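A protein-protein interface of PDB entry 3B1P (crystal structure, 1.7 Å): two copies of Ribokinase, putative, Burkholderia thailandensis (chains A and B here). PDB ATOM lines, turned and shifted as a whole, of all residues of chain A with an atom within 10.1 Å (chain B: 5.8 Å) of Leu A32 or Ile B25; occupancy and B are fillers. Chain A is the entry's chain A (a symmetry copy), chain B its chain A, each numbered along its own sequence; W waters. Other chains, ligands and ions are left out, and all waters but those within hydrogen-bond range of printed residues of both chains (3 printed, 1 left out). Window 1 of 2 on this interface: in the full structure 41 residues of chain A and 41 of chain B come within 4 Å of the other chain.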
ATOM      1  N   ARG A  20      -8.689 -11.226 -22.198  1.00  0.00           N
ATOM      2  CA  ARG A  20      -7.478 -11.885 -22.693  1.00  0.00           C
ATOM      3  C   ARG A  20      -6.540 -12.075 -21.515  1.00  0.00           C
ATOM      4  O   ARG A  20      -6.109 -11.084 -20.902  1.00  0.00           O
ATOM      5  CB  ARG A  20      -6.813 -11.013 -23.783  1.00  0.00           C
ATOM      6  CG  ARG A  20      -7.790 -10.877 -24.980  1.00  0.00           C
ATOM      7  CD  ARG A  20      -7.222 -10.411 -26.311  1.00  0.00           C
ATOM      8  NE  ARG A  20      -7.997 -11.072 -27.390  1.00  0.00           N
ATOM      9  CZ  ARG A  20      -9.318 -10.934 -27.615  1.00  0.00           C
ATOM     10  NH1 ARG A  20      -9.877 -11.613 -28.597  1.00  0.00           N
ATOM     11  NH2 ARG A  20     -10.092 -10.125 -26.875  1.00  0.00           N
ATOM     12  N   PHE A  21      -6.251 -13.340 -21.186  1.00  0.00           N
ATOM     13  CA  PHE A  21      -5.318 -13.586 -20.053  1.00  0.00           C
ATOM     14  C   PHE A  21      -3.989 -12.854 -20.281  1.00  0.00           C
ATOM     15  O   PHE A  21      -3.317 -12.455 -19.311  1.00  0.00           O
ATOM     16  CB  PHE A  21      -5.034 -15.086 -19.871  1.00  0.00           C
ATOM     17  CG  PHE A  21      -6.217 -15.930 -19.464  1.00  0.00           C
ATOM     18  CD1 PHE A  21      -6.293 -17.278 -19.873  1.00  0.00           C
ATOM     19  CD2 PHE A  21      -7.259 -15.418 -18.695  1.00  0.00           C
ATOM     20  CE1 PHE A  21      -7.355 -18.068 -19.480  1.00  0.00           C
ATOM     21  CE2 PHE A  21      -8.355 -16.229 -18.321  1.00  0.00           C
ATOM     22  CZ  PHE A  21      -8.379 -17.559 -18.744  1.00  0.00           C
ATOM     23  N   ARG A  22      -3.551 -12.704 -21.547  1.00  0.00           N
ATOM     24  CA  ARG A  22      -2.274 -12.021 -21.846  1.00  0.00           C
ATOM     25  C   ARG A  22      -2.153 -10.663 -21.114  1.00  0.00           C
ATOM     26  O   ARG A  22      -1.063 -10.297 -20.665  1.00  0.00           O
ATOM     27  CB  ARG A  22      -2.135 -11.781 -23.357  1.00  0.00           C
ATOM     28  CG  ARG A  22      -0.765 -11.300 -23.753  1.00  0.00           C
ATOM     29  CD  ARG A  22      -0.675 -11.122 -25.270  1.00  0.00           C
ATOM     30  NE  ARG A  22      -0.787 -12.405 -25.974  1.00  0.00           N
ATOM     31  CZ  ARG A  22       0.226 -13.225 -26.230  1.00  0.00           C
ATOM     32  NH1 ARG A  22       1.450 -12.942 -25.818  1.00  0.00           N
ATOM     33  NH2 ARG A  22      -0.007 -14.356 -26.907  1.00  0.00           N
ATOM     34  N   GLU A  23      -3.277  -9.929 -21.034  1.00  0.00           N
ATOM     35  CA  GLU A  23      -3.270  -8.562 -20.491  1.00  0.00           C
ATOM     36  C   GLU A  23      -3.154  -8.557 -18.962  1.00  0.00           C
ATOM     37  O   GLU A  23      -2.993  -7.486 -18.325  1.00  0.00           O
ATOM     38  CB  GLU A  23      -4.569  -7.847 -20.850  1.00  0.00           C
ATOM     39  CG  GLU A  23      -4.672  -7.531 -22.325  1.00  0.00           C
ATOM     40  CD  GLU A  23      -6.133  -7.212 -22.722  1.00  0.00           C
ATOM     41  OE1 GLU A  23      -6.986  -6.959 -21.833  1.00  0.00           O
ATOM     42  OE2 GLU A  23      -6.451  -7.282 -23.925  1.00  0.00           O
ATOM     43  N   HIS A  24      -3.184  -9.735 -18.384  1.00  0.00           N
ATOM     44  CA  HIS A  24      -3.265  -9.885 -16.926  1.00  0.00           C
ATOM     45  C   HIS A  24      -2.117 -10.685 -16.334  1.00  0.00           C
ATOM     46  O   HIS A  24      -2.123 -11.000 -15.117  1.00  0.00           O
ATOM     47  CB  HIS A  24      -4.581 -10.581 -16.603  1.00  0.00           C
ATOM     48  CG  HIS A  24      -5.773  -9.752 -16.974  1.00  0.00           C
ATOM     49  ND1 HIS A  24      -6.198  -8.672 -16.217  1.00  0.00           N
ATOM     50  CD2 HIS A  24      -6.545  -9.758 -18.087  1.00  0.00           C
ATOM     51  CE1 HIS A  24      -7.241  -8.105 -16.813  1.00  0.00           C
ATOM     52  NE2 HIS A  24      -7.460  -8.729 -17.959  1.00  0.00           N
ATOM     53  N   ILE A  25      -1.175 -11.087 -17.181  1.00  0.00           N
ATOM     54  CA  ILE A  25      -0.023 -11.855 -16.701  1.00  0.00           C
ATOM     55  C   ILE A  25       1.144 -10.909 -16.452  1.00  0.00           C
ATOM     56  O   ILE A  25       1.529 -10.097 -17.360  1.00  0.00           O
ATOM     57  CB  ILE A  25       0.331 -12.940 -17.738  1.00  0.00           C
ATOM     58  CG1 ILE A  25      -0.794 -13.954 -17.778  1.00  0.00           C
ATOM     59  CG2 ILE A  25       1.712 -13.587 -17.419  1.00  0.00           C
ATOM     60  CD1 ILE A  25      -0.715 -14.953 -18.968  1.00  0.00           C
ATOM     61  N   LEU A  26       1.700 -10.974 -15.248  1.00  0.00           N
ATOM     62  CA  LEU A  26       2.806 -10.086 -14.859  1.00  0.00           C
ATOM     63  C   LEU A  26       3.987 -10.970 -14.483  1.00  0.00           C
ATOM     64  O   LEU A  26       4.112 -11.434 -13.320  1.00  0.00           O
ATOM     65  CB  LEU A  26       2.389  -9.210 -13.677  1.00  0.00           C
ATOM     66  CG  LEU A  26       1.326  -8.157 -13.841  1.00  0.00           C
ATOM     67  CD1 LEU A  26       1.138  -7.404 -12.489  1.00  0.00           C
ATOM     68  CD2 LEU A  26       1.743  -7.202 -15.004  1.00  0.00           C
ATOM     69  N   PRO A  27       4.846 -11.283 -15.459  1.00  0.00           N
ATOM     70  CA  PRO A  27       5.858 -12.326 -15.217  1.00  0.00           C
ATOM     71  C   PRO A  27       6.865 -11.953 -14.117  1.00  0.00           C
ATOM     72  O   PRO A  27       7.446 -12.844 -13.515  1.00  0.00           O
ATOM     73  CB  PRO A  27       6.626 -12.378 -16.554  1.00  0.00           C
ATOM     74  CG  PRO A  27       5.731 -11.838 -17.521  1.00  0.00           C
ATOM     75  CD  PRO A  27       4.851 -10.813 -16.859  1.00  0.00           C
ATOM     76  N   ASP A  28       7.061 -10.661 -13.869  1.00  0.00           N
ATOM     77  CA  ASP A  28       8.043 -10.190 -12.874  1.00  0.00           C
ATOM     78  C   ASP A  28       7.646 -10.475 -11.427  1.00  0.00           C
ATOM     79  O   ASP A  28       8.491 -10.364 -10.533  1.00  0.00           O
ATOM     80  CB  ASP A  28       8.263  -8.652 -13.002  1.00  0.00           C
ATOM     81  CG  ASP A  28       8.928  -8.252 -14.302  1.00  0.00           C
ATOM     82  OD1 ASP A  28       9.430  -9.131 -15.010  1.00  0.00           O
ATOM     83  OD2 ASP A  28       8.908  -7.022 -14.622  1.00  0.00           O
ATOM     84  N   GLN A  29       6.373 -10.823 -11.191  1.00  0.00           N
ATOM     85  CA  GLN A  29       5.832 -11.032  -9.832  1.00  0.00           C
ATOM     86  C   GLN A  29       5.885 -12.502  -9.456  1.00  0.00           C
ATOM     87  O   GLN A  29       5.936 -13.396 -10.316  1.00  0.00           O
ATOM     88  CB  GLN A  29       4.392 -10.485  -9.728  1.00  0.00           C
ATOM     89  CG  GLN A  29       4.251  -8.967 -10.029  1.00  0.00           C
ATOM     90  CD  GLN A  29       5.304  -8.173  -9.335  1.00  0.00           C
ATOM     91  OE1 GLN A  29       5.470  -8.282  -8.115  1.00  0.00           O
ATOM     92  NE2 GLN A  29       6.070  -7.403 -10.102  1.00  0.00           N
ATOM     93  N   VAL A  30       5.924 -12.791  -8.151  1.00  0.00           N
ATOM     94  CA  VAL A  30       5.881 -14.170  -7.687  1.00  0.00           C
ATOM     95  C   VAL A  30       4.559 -14.863  -8.090  1.00  0.00           C
ATOM     96  O   VAL A  30       4.548 -16.055  -8.510  1.00  0.00           O
ATOM     97  CB  VAL A  30       6.058 -14.246  -6.132  1.00  0.00           C
ATOM     98  CG1 VAL A  30       5.795 -15.670  -5.630  1.00  0.00           C
ATOM     99  CG2 VAL A  30       7.433 -13.729  -5.773  1.00  0.00           C
ATOM    100  N   HIS A  31       3.457 -14.111  -7.978  1.00  0.00           N
ATOM    101  CA  HIS A  31       2.171 -14.506  -8.546  1.00  0.00           C
ATOM    102  C   HIS A  31       2.046 -13.840  -9.895  1.00  0.00           C
ATOM    103  O   HIS A  31       1.966 -12.649  -9.961  1.00  0.00           O
ATOM    104  CB  HIS A  31       1.018 -14.011  -7.682  1.00  0.00           C
ATOM    105  CG  HIS A  31       1.111 -14.455  -6.256  1.00  0.00           C
ATOM    106  ND1 HIS A  31       1.869 -13.771  -5.326  1.00  0.00           N
ATOM    107  CD2 HIS A  31       0.477 -15.450  -5.583  1.00  0.00           C
ATOM    108  CE1 HIS A  31       1.741 -14.369  -4.140  1.00  0.00           C
ATOM    109  NE2 HIS A  31       0.914 -15.398  -4.274  1.00  0.00           N
ATOM    110  N   LEU A  32       2.057 -14.612 -10.986  1.00  0.00           N
ATOM    111  CA  LEU A  32       2.028 -13.977 -12.291  1.00  0.00           C
ATOM    112  C   LEU A  32       0.589 -13.701 -12.771  1.00  0.00           C
ATOM    113  O   LEU A  32       0.415 -12.930 -13.689  1.00  0.00           O
ATOM    114  CB  LEU A  32       2.846 -14.818 -13.319  1.00  0.00           C
ATOM    115  CG  LEU A  32       2.471 -16.258 -13.606  1.00  0.00           C
ATOM    116  CD1 LEU A  32       1.268 -16.273 -14.521  1.00  0.00           C
ATOM    117  CD2 LEU A  32       3.593 -16.960 -14.360  1.00  0.00           C
ATOM    118  N   ILE A  33      -0.420 -14.320 -12.162  1.00  0.00           N
ATOM    119  CA  ILE A  33      -1.826 -13.983 -12.530  1.00  0.00           C
ATOM    120  C   ILE A  33      -2.742 -14.285 -11.363  1.00  0.00           C
ATOM    121  O   ILE A  33      -2.652 -15.359 -10.757  1.00  0.00           O
ATOM    122  CB  ILE A  33      -2.338 -14.707 -13.819  1.00  0.00           C
ATOM    123  CG1 ILE A  33      -3.737 -14.170 -14.174  1.00  0.00           C
ATOM    124  CG2 ILE A  33      -2.321 -16.202 -13.655  1.00  0.00           C
ATOM    125  CD1 ILE A  33      -4.153 -14.505 -15.598  1.00  0.00           C
ATOM    126  N   ASN A  34      -3.550 -13.294 -11.021  1.00  0.00           N
ATOM    127  CA  ASN A  34      -4.690 -13.494 -10.117  1.00  0.00           C
ATOM    128  C   ASN A  34      -5.875 -12.865 -10.825  1.00  0.00           C
ATOM    129  O   ASN A  34      -5.841 -11.641 -11.157  1.00  0.00           O
ATOM    130  CB  ASN A  34      -4.497 -12.630  -8.875  1.00  0.00           C
ATOM    131  CG  ASN A  34      -3.682 -13.277  -7.804  1.00  0.00           C
ATOM    132  OD1 ASN A  34      -3.145 -14.388  -7.931  1.00  0.00           O
ATOM    133  ND2 ASN A  34      -3.565 -12.557  -6.721  1.00  0.00           N
ATOM    134  N   LEU A  35      -6.906 -13.643 -11.124  1.00  0.00           N
ATOM    135  CA  LEU A  35      -8.027 -13.059 -11.874  1.00  0.00           C
ATOM    136  C   LEU A  35      -9.288 -13.760 -11.452  1.00  0.00           C
ATOM    137  O   LEU A  35      -9.351 -14.967 -11.542  1.00  0.00           O
ATOM    138  CB  LEU A  35      -7.807 -13.289 -13.405  1.00  0.00           C
ATOM    139  CG  LEU A  35      -8.901 -12.833 -14.346  1.00  0.00           C
ATOM    140  CD1 LEU A  35      -9.060 -11.295 -14.233  1.00  0.00           C
ATOM    141  CD2 LEU A  35      -8.487 -13.320 -15.770  1.00  0.00           C
ATOM    142  N   ASN A 112      -7.004 -19.597 -24.884  1.00  0.00           N
ATOM    143  CA  ASN A 112      -6.102 -20.197 -23.889  1.00  0.00           C
ATOM    144  C   ASN A 112      -6.765 -21.139 -22.831  1.00  0.00           C
ATOM    145  O   ASN A 112      -7.143 -20.731 -21.693  1.00  0.00           O
ATOM    146  CB  ASN A 112      -5.397 -19.096 -23.145  1.00  0.00           C
ATOM    147  CG  ASN A 112      -4.462 -18.270 -24.053  1.00  0.00           C
ATOM    148  OD1 ASN A 112      -3.613 -18.819 -24.730  1.00  0.00           O
ATOM    149  ND2 ASN A 112      -4.607 -16.954 -24.035  1.00  0.00           N
ATOM    150  N   GLN A 113      -6.820 -22.399 -23.096  1.00  0.00           N
ATOM    151  CA  GLN A 113      -7.641 -23.246 -22.273  1.00  0.00           C
ATOM    152  C   GLN A 113      -6.785 -23.820 -21.196  1.00  0.00           C
ATOM    153  O   GLN A 113      -5.759 -24.474 -21.489  1.00  0.00           O
ATOM    154  CB  GLN A 113      -8.257 -24.367 -23.111  1.00  0.00           C
ATOM    155  CG  GLN A 113      -9.097 -23.769 -24.235  1.00  0.00           C
ATOM    156  CD  GLN A 113     -10.324 -24.562 -24.461  1.00  0.00           C
ATOM    157  OE1 GLN A 113     -10.295 -25.819 -24.507  1.00  0.00           O
ATOM    158  NE2 GLN A 113     -11.449 -23.846 -24.578  1.00  0.00           N
ATOM    159  N   ILE A 114      -7.247 -23.623 -19.949  1.00  0.00           N
ATOM    160  CA  ILE A 114      -6.674 -24.394 -18.828  1.00  0.00           C
ATOM    161  C   ILE A 114      -7.799 -25.320 -18.303  1.00  0.00           C
ATOM    162  O   ILE A 114      -8.808 -24.830 -17.817  1.00  0.00           O
ATOM    163  CB  ILE A 114      -6.153 -23.443 -17.739  1.00  0.00           C
ATOM    164  CG1 ILE A 114      -5.031 -22.522 -18.284  1.00  0.00           C
ATOM    165  CG2 ILE A 114      -5.644 -24.282 -16.537  1.00  0.00           C
ATOM    166  CD1 ILE A 114      -4.635 -21.371 -17.330  1.00  0.00           C
ATOM    167  N   TYR A 194       0.575 -23.364 -30.392  1.00  0.00           N
ATOM    168  CA  TYR A 194       1.197 -23.684 -29.105  1.00  0.00           C
ATOM    169  C   TYR A 194       1.583 -25.169 -29.106  1.00  0.00           C
ATOM    170  O   TYR A 194       2.746 -25.523 -28.759  1.00  0.00           O
ATOM    171  CB  TYR A 194       0.211 -23.389 -27.998  1.00  0.00           C
ATOM    172  CG  TYR A 194       0.634 -23.788 -26.586  1.00  0.00           C
ATOM    173  CD1 TYR A 194       0.402 -25.075 -26.088  1.00  0.00           C
ATOM    174  CD2 TYR A 194       1.178 -22.807 -25.739  1.00  0.00           C
ATOM    175  CE1 TYR A 194       0.781 -25.419 -24.806  1.00  0.00           C
ATOM    176  CE2 TYR A 194       1.530 -23.133 -24.433  1.00  0.00           C
ATOM    177  CZ  TYR A 194       1.329 -24.415 -23.985  1.00  0.00           C
ATOM    178  OH  TYR A 194       1.716 -24.747 -22.690  1.00  0.00           O
ATOM    179  N   LYS A 197       4.672 -25.928 -31.135  1.00  0.00           N
ATOM    180  CA  LYS A 197       5.965 -25.620 -30.456  1.00  0.00           C
ATOM    181  C   LYS A 197       6.286 -26.753 -29.499  1.00  0.00           C
ATOM    182  O   LYS A 197       7.455 -27.206 -29.433  1.00  0.00           O
ATOM    183  CB  LYS A 197       5.900 -24.303 -29.670  1.00  0.00           C
ATOM    184  CG  LYS A 197       6.179 -23.086 -30.530  1.00  0.00           C
ATOM    185  CD  LYS A 197       7.608 -23.113 -31.137  1.00  0.00           C
ATOM    186  CE  LYS A 197       8.667 -22.753 -30.103  1.00  0.00           C
ATOM    187  NZ  LYS A 197      10.000 -22.482 -30.684  1.00  0.00           N
ATOM    188  N   LEU A 198       5.267 -27.236 -28.785  1.00  0.00           N
ATOM    189  CA  LEU A 198       5.492 -28.376 -27.870  1.00  0.00           C
ATOM    190  C   LEU A 198       5.915 -29.658 -28.611  1.00  0.00           C
ATOM    191  O   LEU A 198       6.760 -30.418 -28.132  1.00  0.00           O
ATOM    192  CB  LEU A 198       4.256 -28.661 -27.038  1.00  0.00           C
ATOM    193  CG  LEU A 198       4.076 -27.930 -25.695  1.00  0.00           C
ATOM    194  CD1 LEU A 198       4.551 -26.526 -25.682  1.00  0.00           C
ATOM    195  CD2 LEU A 198       2.629 -28.128 -25.282  1.00  0.00           C
ATOM    196  N   PHE B  21       2.124 -22.867 -13.639  1.00  0.00           N
ATOM    197  CA  PHE B  21       1.687 -22.331 -14.957  1.00  0.00           C
ATOM    198  C   PHE B  21       2.847 -21.610 -15.657  1.00  0.00           C
ATOM    199  O   PHE B  21       2.909 -21.580 -16.900  1.00  0.00           O
ATOM    200  CB  PHE B  21       0.512 -21.352 -14.807  1.00  0.00           C
ATOM    201  CG  PHE B  21      -0.775 -21.950 -14.293  1.00  0.00           C
ATOM    202  CD1 PHE B  21      -1.659 -21.163 -13.527  1.00  0.00           C
ATOM    203  CD2 PHE B  21      -1.124 -23.274 -14.543  1.00  0.00           C
ATOM    204  CE1 PHE B  21      -2.854 -21.690 -13.078  1.00  0.00           C
ATOM    205  CE2 PHE B  21      -2.338 -23.812 -14.057  1.00  0.00           C
ATOM    206  CZ  PHE B  21      -3.184 -22.989 -13.310  1.00  0.00           C
ATOM    207  N   ARG B  22       3.757 -20.973 -14.893  1.00  0.00           N
ATOM    208  CA  ARG B  22       4.895 -20.245 -15.494  1.00  0.00           C
ATOM    209  C   ARG B  22       5.641 -21.098 -16.549  1.00  0.00           C
ATOM    210  O   ARG B  22       6.087 -20.567 -17.570  1.00  0.00           O
ATOM    211  CB  ARG B  22       5.895 -19.821 -14.408  1.00  0.00           C
ATOM    212  CG  ARG B  22       6.955 -18.883 -14.917  1.00  0.00           C
ATOM    213  CD  ARG B  22       7.892 -18.462 -13.782  1.00  0.00           C
ATOM    214  NE  ARG B  22       7.195 -17.651 -12.776  1.00  0.00           N
ATOM    215  CZ  ARG B  22       7.033 -16.334 -12.838  1.00  0.00           C
ATOM    216  NH1 ARG B  22       7.478 -15.642 -13.872  1.00  0.00           N
ATOM    217  NH2 ARG B  22       6.399 -15.709 -11.838  1.00  0.00           N
ATOM    218  N   GLU B  23       5.784 -22.404 -16.264  1.00  0.00           N
ATOM    219  CA  GLU B  23       6.593 -23.295 -17.111  1.00  0.00           C
ATOM    220  C   GLU B  23       5.867 -23.656 -18.413  1.00  0.00           C
ATOM    221  O   GLU B  23       6.448 -24.294 -19.326  1.00  0.00           O
ATOM    222  CB  GLU B  23       6.881 -24.600 -16.374  1.00  0.00           C
ATOM    223  CG  GLU B  23       7.837 -24.418 -15.218  1.00  0.00           C
ATOM    224  CD  GLU B  23       7.775 -25.627 -14.253  1.00  0.00           C
ATOM    225  OE1 GLU B  23       7.227 -26.697 -14.619  1.00  0.00           O
ATOM    226  OE2 GLU B  23       8.214 -25.485 -13.094  1.00  0.00           O
ATOM    227  N   HIS B  24       4.636 -23.215 -18.520  1.00  0.00           N
ATOM    228  CA  HIS B  24       3.754 -23.626 -19.619  1.00  0.00           C
ATOM    229  C   HIS B  24       3.229 -22.463 -20.444  1.00  0.00           C
ATOM    230  O   HIS B  24       2.365 -22.656 -21.336  1.00  0.00           O
ATOM    231  CB  HIS B  24       2.580 -24.385 -19.015  1.00  0.00           C
ATOM    232  CG  HIS B  24       3.003 -25.663 -18.356  1.00  0.00           C
ATOM    233  ND1 HIS B  24       3.324 -26.803 -19.075  1.00  0.00           N
ATOM    234  CD2 HIS B  24       3.287 -25.941 -17.061  1.00  0.00           C
ATOM    235  CE1 HIS B  24       3.705 -27.756 -18.232  1.00  0.00           C
ATOM    236  NE2 HIS B  24       3.712 -27.257 -17.007  1.00  0.00           N
ATOM    237  N   ILE B  25       3.669 -21.253 -20.111  1.00  0.00           N
ATOM    238  CA  ILE B  25       3.226 -20.072 -20.856  1.00  0.00           C
ATOM    239  C   ILE B  25       4.258 -19.734 -21.923  1.00  0.00           C
ATOM    240  O   ILE B  25       5.491 -19.601 -21.620  1.00  0.00           O
ATOM    241  CB  ILE B  25       3.017 -18.902 -19.873  1.00  0.00           C
ATOM    242  CG1 ILE B  25       1.842 -19.232 -18.976  1.00  0.00           C
ATOM    243  CG2 ILE B  25       2.831 -17.558 -20.637  1.00  0.00           C
ATOM    244  CD1 ILE B  25       1.680 -18.281 -17.755  1.00  0.00           C
ATOM    245  N   LEU B  26       3.795 -19.614 -23.163  1.00  0.00           N
ATOM    246  CA  LEU B  26       4.689 -19.335 -24.297  1.00  0.00           C
ATOM    247  C   LEU B  26       4.217 -18.037 -24.938  1.00  0.00           C
ATOM    248  O   LEU B  26       3.310 -18.030 -25.809  1.00  0.00           O
ATOM    249  CB  LEU B  26       4.638 -20.484 -25.304  1.00  0.00           C
ATOM    250  CG  LEU B  26       5.178 -21.842 -24.946  1.00  0.00           C
ATOM    251  CD1 LEU B  26       5.025 -22.795 -26.170  1.00  0.00           C
ATOM    252  CD2 LEU B  26       6.664 -21.686 -24.492  1.00  0.00           C
ATOM    253  N   PRO B  27       4.764 -16.903 -24.486  1.00  0.00           N
ATOM    254  CA  PRO B  27       4.174 -15.613 -24.885  1.00  0.00           C
ATOM    255  C   PRO B  27       4.269 -15.343 -26.395  1.00  0.00           C
ATOM    256  O   PRO B  27       3.467 -14.581 -26.914  1.00  0.00           O
ATOM    257  CB  PRO B  27       5.077 -14.586 -24.170  1.00  0.00           C
ATOM    258  CG  PRO B  27       5.675 -15.299 -23.093  1.00  0.00           C
ATOM    259  CD  PRO B  27       5.841 -16.741 -23.489  1.00  0.00           C
ATOM    260  N   LEU B  32      -1.096 -18.625 -25.734  1.00  0.00           N
ATOM    261  CA  LEU B  32       0.052 -18.606 -24.847  1.00  0.00           C
ATOM    262  C   LEU B  32       0.005 -19.750 -23.813  1.00  0.00           C
ATOM    263  O   LEU B  32       1.014 -20.032 -23.207  1.00  0.00           O
ATOM    264  CB  LEU B  32       0.193 -17.205 -24.176  1.00  0.00           C
ATOM    265  CG  LEU B  32      -0.930 -16.640 -23.332  1.00  0.00           C
ATOM    266  CD1 LEU B  32      -0.904 -17.312 -21.978  1.00  0.00           C
ATOM    267  CD2 LEU B  32      -0.710 -15.154 -23.077  1.00  0.00           C
ATOM    268  N   ILE B  33      -1.145 -20.391 -23.618  1.00  0.00           N
ATOM    269  CA  ILE B  33      -1.187 -21.574 -22.710  1.00  0.00           C
ATOM    270  C   ILE B  33      -2.336 -22.477 -23.107  1.00  0.00           C
ATOM    271  O   ILE B  33      -3.457 -22.005 -23.329  1.00  0.00           O
ATOM    272  CB  ILE B  33      -1.290 -21.209 -21.192  1.00  0.00           C
ATOM    273  CG1 ILE B  33      -1.179 -22.497 -20.358  1.00  0.00           C
ATOM    274  CG2 ILE B  33      -2.547 -20.437 -20.894  1.00  0.00           C
ATOM    275  CD1 ILE B  33      -0.872 -22.227 -18.892  1.00  0.00           C
ATOM    276  N   ASN B 112      -1.216 -19.000  -8.416  1.00  0.00           N
ATOM    277  CA  ASN B 112      -1.873 -18.257  -9.502  1.00  0.00           C
ATOM    278  C   ASN B 112      -3.382 -18.583  -9.751  1.00  0.00           C
ATOM    279  O   ASN B 112      -3.766 -19.436 -10.604  1.00  0.00           O
ATOM    280  CB  ASN B 112      -1.131 -18.513 -10.785  1.00  0.00           C
ATOM    281  CG  ASN B 112       0.307 -17.953 -10.761  1.00  0.00           C
ATOM    282  OD1 ASN B 112       0.513 -16.789 -10.478  1.00  0.00           O
ATOM    283  ND2 ASN B 112       1.285 -18.783 -11.090  1.00  0.00           N
ATOM    284  N   TYR B 194       1.250  -9.367  -6.652  1.00  0.00           N
ATOM    285  CA  TYR B 194       0.568  -9.083  -7.916  1.00  0.00           C
ATOM    286  C   TYR B 194      -0.468  -7.977  -7.673  1.00  0.00           C
ATOM    287  O   TYR B 194      -0.513  -6.970  -8.436  1.00  0.00           O
ATOM    288  CB  TYR B 194      -0.104 -10.346  -8.405  1.00  0.00           C
ATOM    289  CG  TYR B 194      -0.980 -10.212  -9.648  1.00  0.00           C
ATOM    290  CD1 TYR B 194      -2.328  -9.847  -9.557  1.00  0.00           C
ATOM    291  CD2 TYR B 194      -0.442 -10.561 -10.898  1.00  0.00           C
ATOM    292  CE1 TYR B 194      -3.113  -9.740 -10.688  1.00  0.00           C
ATOM    293  CE2 TYR B 194      -1.233 -10.491 -12.040  1.00  0.00           C
ATOM    294  CZ  TYR B 194      -2.542 -10.090 -11.926  1.00  0.00           C
ATOM    295  OH  TYR B 194      -3.320  -9.987 -13.075  1.00  0.00           O
HETATM  296  O   HOH W   1      -4.984  -7.893 -13.930  1.00  0.00           O
HETATM  297  O   HOH W   2       4.114 -17.663 -10.581  1.00  0.00           O
HETATM  298  O   HOH W   3       3.213 -26.937 -21.773  1.00  0.00           O
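Leu B32 touches Arg A22.
Val A30 touches Arg B22 (O to NH2, 3.8 Å).
His A31 touches Tyr B194 (O to CD2, 3.3 Å).
Leu A32 touches Arg B22 (CD2 to CB, 3.7 Å).
CD1 of Leu A32 touches CD1 of Ile B25, at 3.8 Å.
Tyr B194 touches Leu A32.
CE2 of Tyr B194 touches CA of Ile A33 (3.6 Å).
CE2 of Tyr A194 touches O of Leu B32, at 3.4 Å.
CA of Ile B33 touches CE2 of Tyr A194, at 3.6 Å.
CD1 of Leu B26 touches CB of Lys A197, at 3.9 Å.
Printed residues of chain B within 4 Å of Leu A26: Tyr B194 (3.9 Å).
Leu A32 touches just these residues of chain B: Arg B22 (3.7 Å), Ile B25 (3.8 Å), Asn B112 (2.7 Å) and Tyr B194 (3.4 Å).
Of the printed residues of chain B, Ile A33 touches Asn B112 and Tyr B194.
Ile A114 touches none of the printed residues of chain B.
Printed residues of chain B within 4 Å of Leu A198: Leu B26.
Arg B22 touches just these residues of chain A: Pro A27 (2.8 Å), Gln A29 (2.8 Å), Val A30 (3.8 Å) and Leu A32 (3.7 Å).
Of chain A, only Leu A32 (3.8 Å) comes within 4 Å of Ile B25.
Of chain A, only Tyr A194 (3.9 Å), Lys A197 (3.9 Å) and Leu A198 (3.8 Å) come within 4 Å of Leu B26.
Printed residues of chain A within 4 Å of Tyr B194: His A24, Leu A26, His A31, Leu A32, Ile A33 and Asn A34.
The nearest residue of chain B that does not touch Leu A32 is Phe B21 (4.9 Å).
The nearest residue of chain A that does not touch Ile B25 is Ile A25 (4.3 Å).
Of the 22 printed residues of chain A, 16 touch a printed residue of chain B.
Printed residues of chain A that touch a printed residue of chain B: Arg A22, His A24, Ile A25, Leu A26, Pro A27, Gln A29, Val A30, His A31, Leu A32, Ile A33, Asn A34, Asn A112, Gln A113, Tyr A194, Lys A197 and Leu A198.
Hydrophobic or aromatic side chains of chain A within 4 Å of the printed part of chain B: His A24, Ile A25, Leu A26, His A31, Leu A32, Ile A33, Tyr A194 and Leu A198.
Arg A22 touches Pro B27, and with the chains exchanged Pro A27 touches Arg B22.
His A24 touches Tyr B194, and with the chains exchanged Tyr A194 touches His B24.
Leu A26 touches Tyr B194, and with the chains exchanged Tyr A194 touches Leu B26.
Leu A32 touches Asn B112, and with the chains exchanged Asn A112 touches Leu B32.
Water W2 lies within hydrogen-bond range of O of Val A30, ND2 of Asn B112 and NH2 of Arg B22.
Water W3 lies within hydrogen-bond range of ND1 of His B24 (2.7 Å) and OH of Tyr A194 (2.8 Å).
Water W1 lies within hydrogen-bond range of a ring nitrogen (ND1) of His A24 and the side-chain hydroxyl of Tyr B194.
The backbone carbonyl oxygen (O) of Leu B32 is in hydrogen-bond range of the backbone NH (N) of Leu B26.
The backbone NH of Leu A26 lies within hydrogen-bond range of the backbone carbonyl oxygen of Leu A32 (2.8 Å).
The guanidinium group (NH1) of Arg B22 sits at hydrogen-bond distance from the backbone carbonyl oxygen (O) of Pro A27 (2.8 Å).
The guanidinium group of Arg B22 sits at hydrogen-bond distance from the backbone carbonyl oxygen of Gln A29, at 2.8 Å.
The backbone carbonyl oxygen (O) of His B24 sits at hydrogen-bond distance from the side-chain hydroxyl (OH) of Tyr A194.
O of Pro B27 sits at hydrogen-bond distance from NH1 of Arg A22, 2.8 Å away.
N of Leu B32 lies within hydrogen-bond range of OD1 of Asn A112, 2.7 Å away.
The backbone NH (N) of Ile B33 is in hydrogen-bond range of the side-chain amide oxygen (OD1) of Asn A112 (3.1 Å).
The backbone carbonyl oxygen (O) of Ile B33 is in hydrogen-bond range of the backbone NH (N) of Gln A113, at 3.4 Å.
The side-chain amide oxygen (OD1) of Asn B112 sits at hydrogen-bond distance from the backbone NH (N) of Leu A32, 2.7 Å away.
The side-chain amide oxygen (OD1) of Asn B112 sits at hydrogen-bond distance from the backbone NH (N) of Ile A33, at 3.1 Å.
The side-chain hydroxyl (OH) of Tyr B194 lies within hydrogen-bond range of the backbone carbonyl oxygen (O) of His A24, 2.6 Å away.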
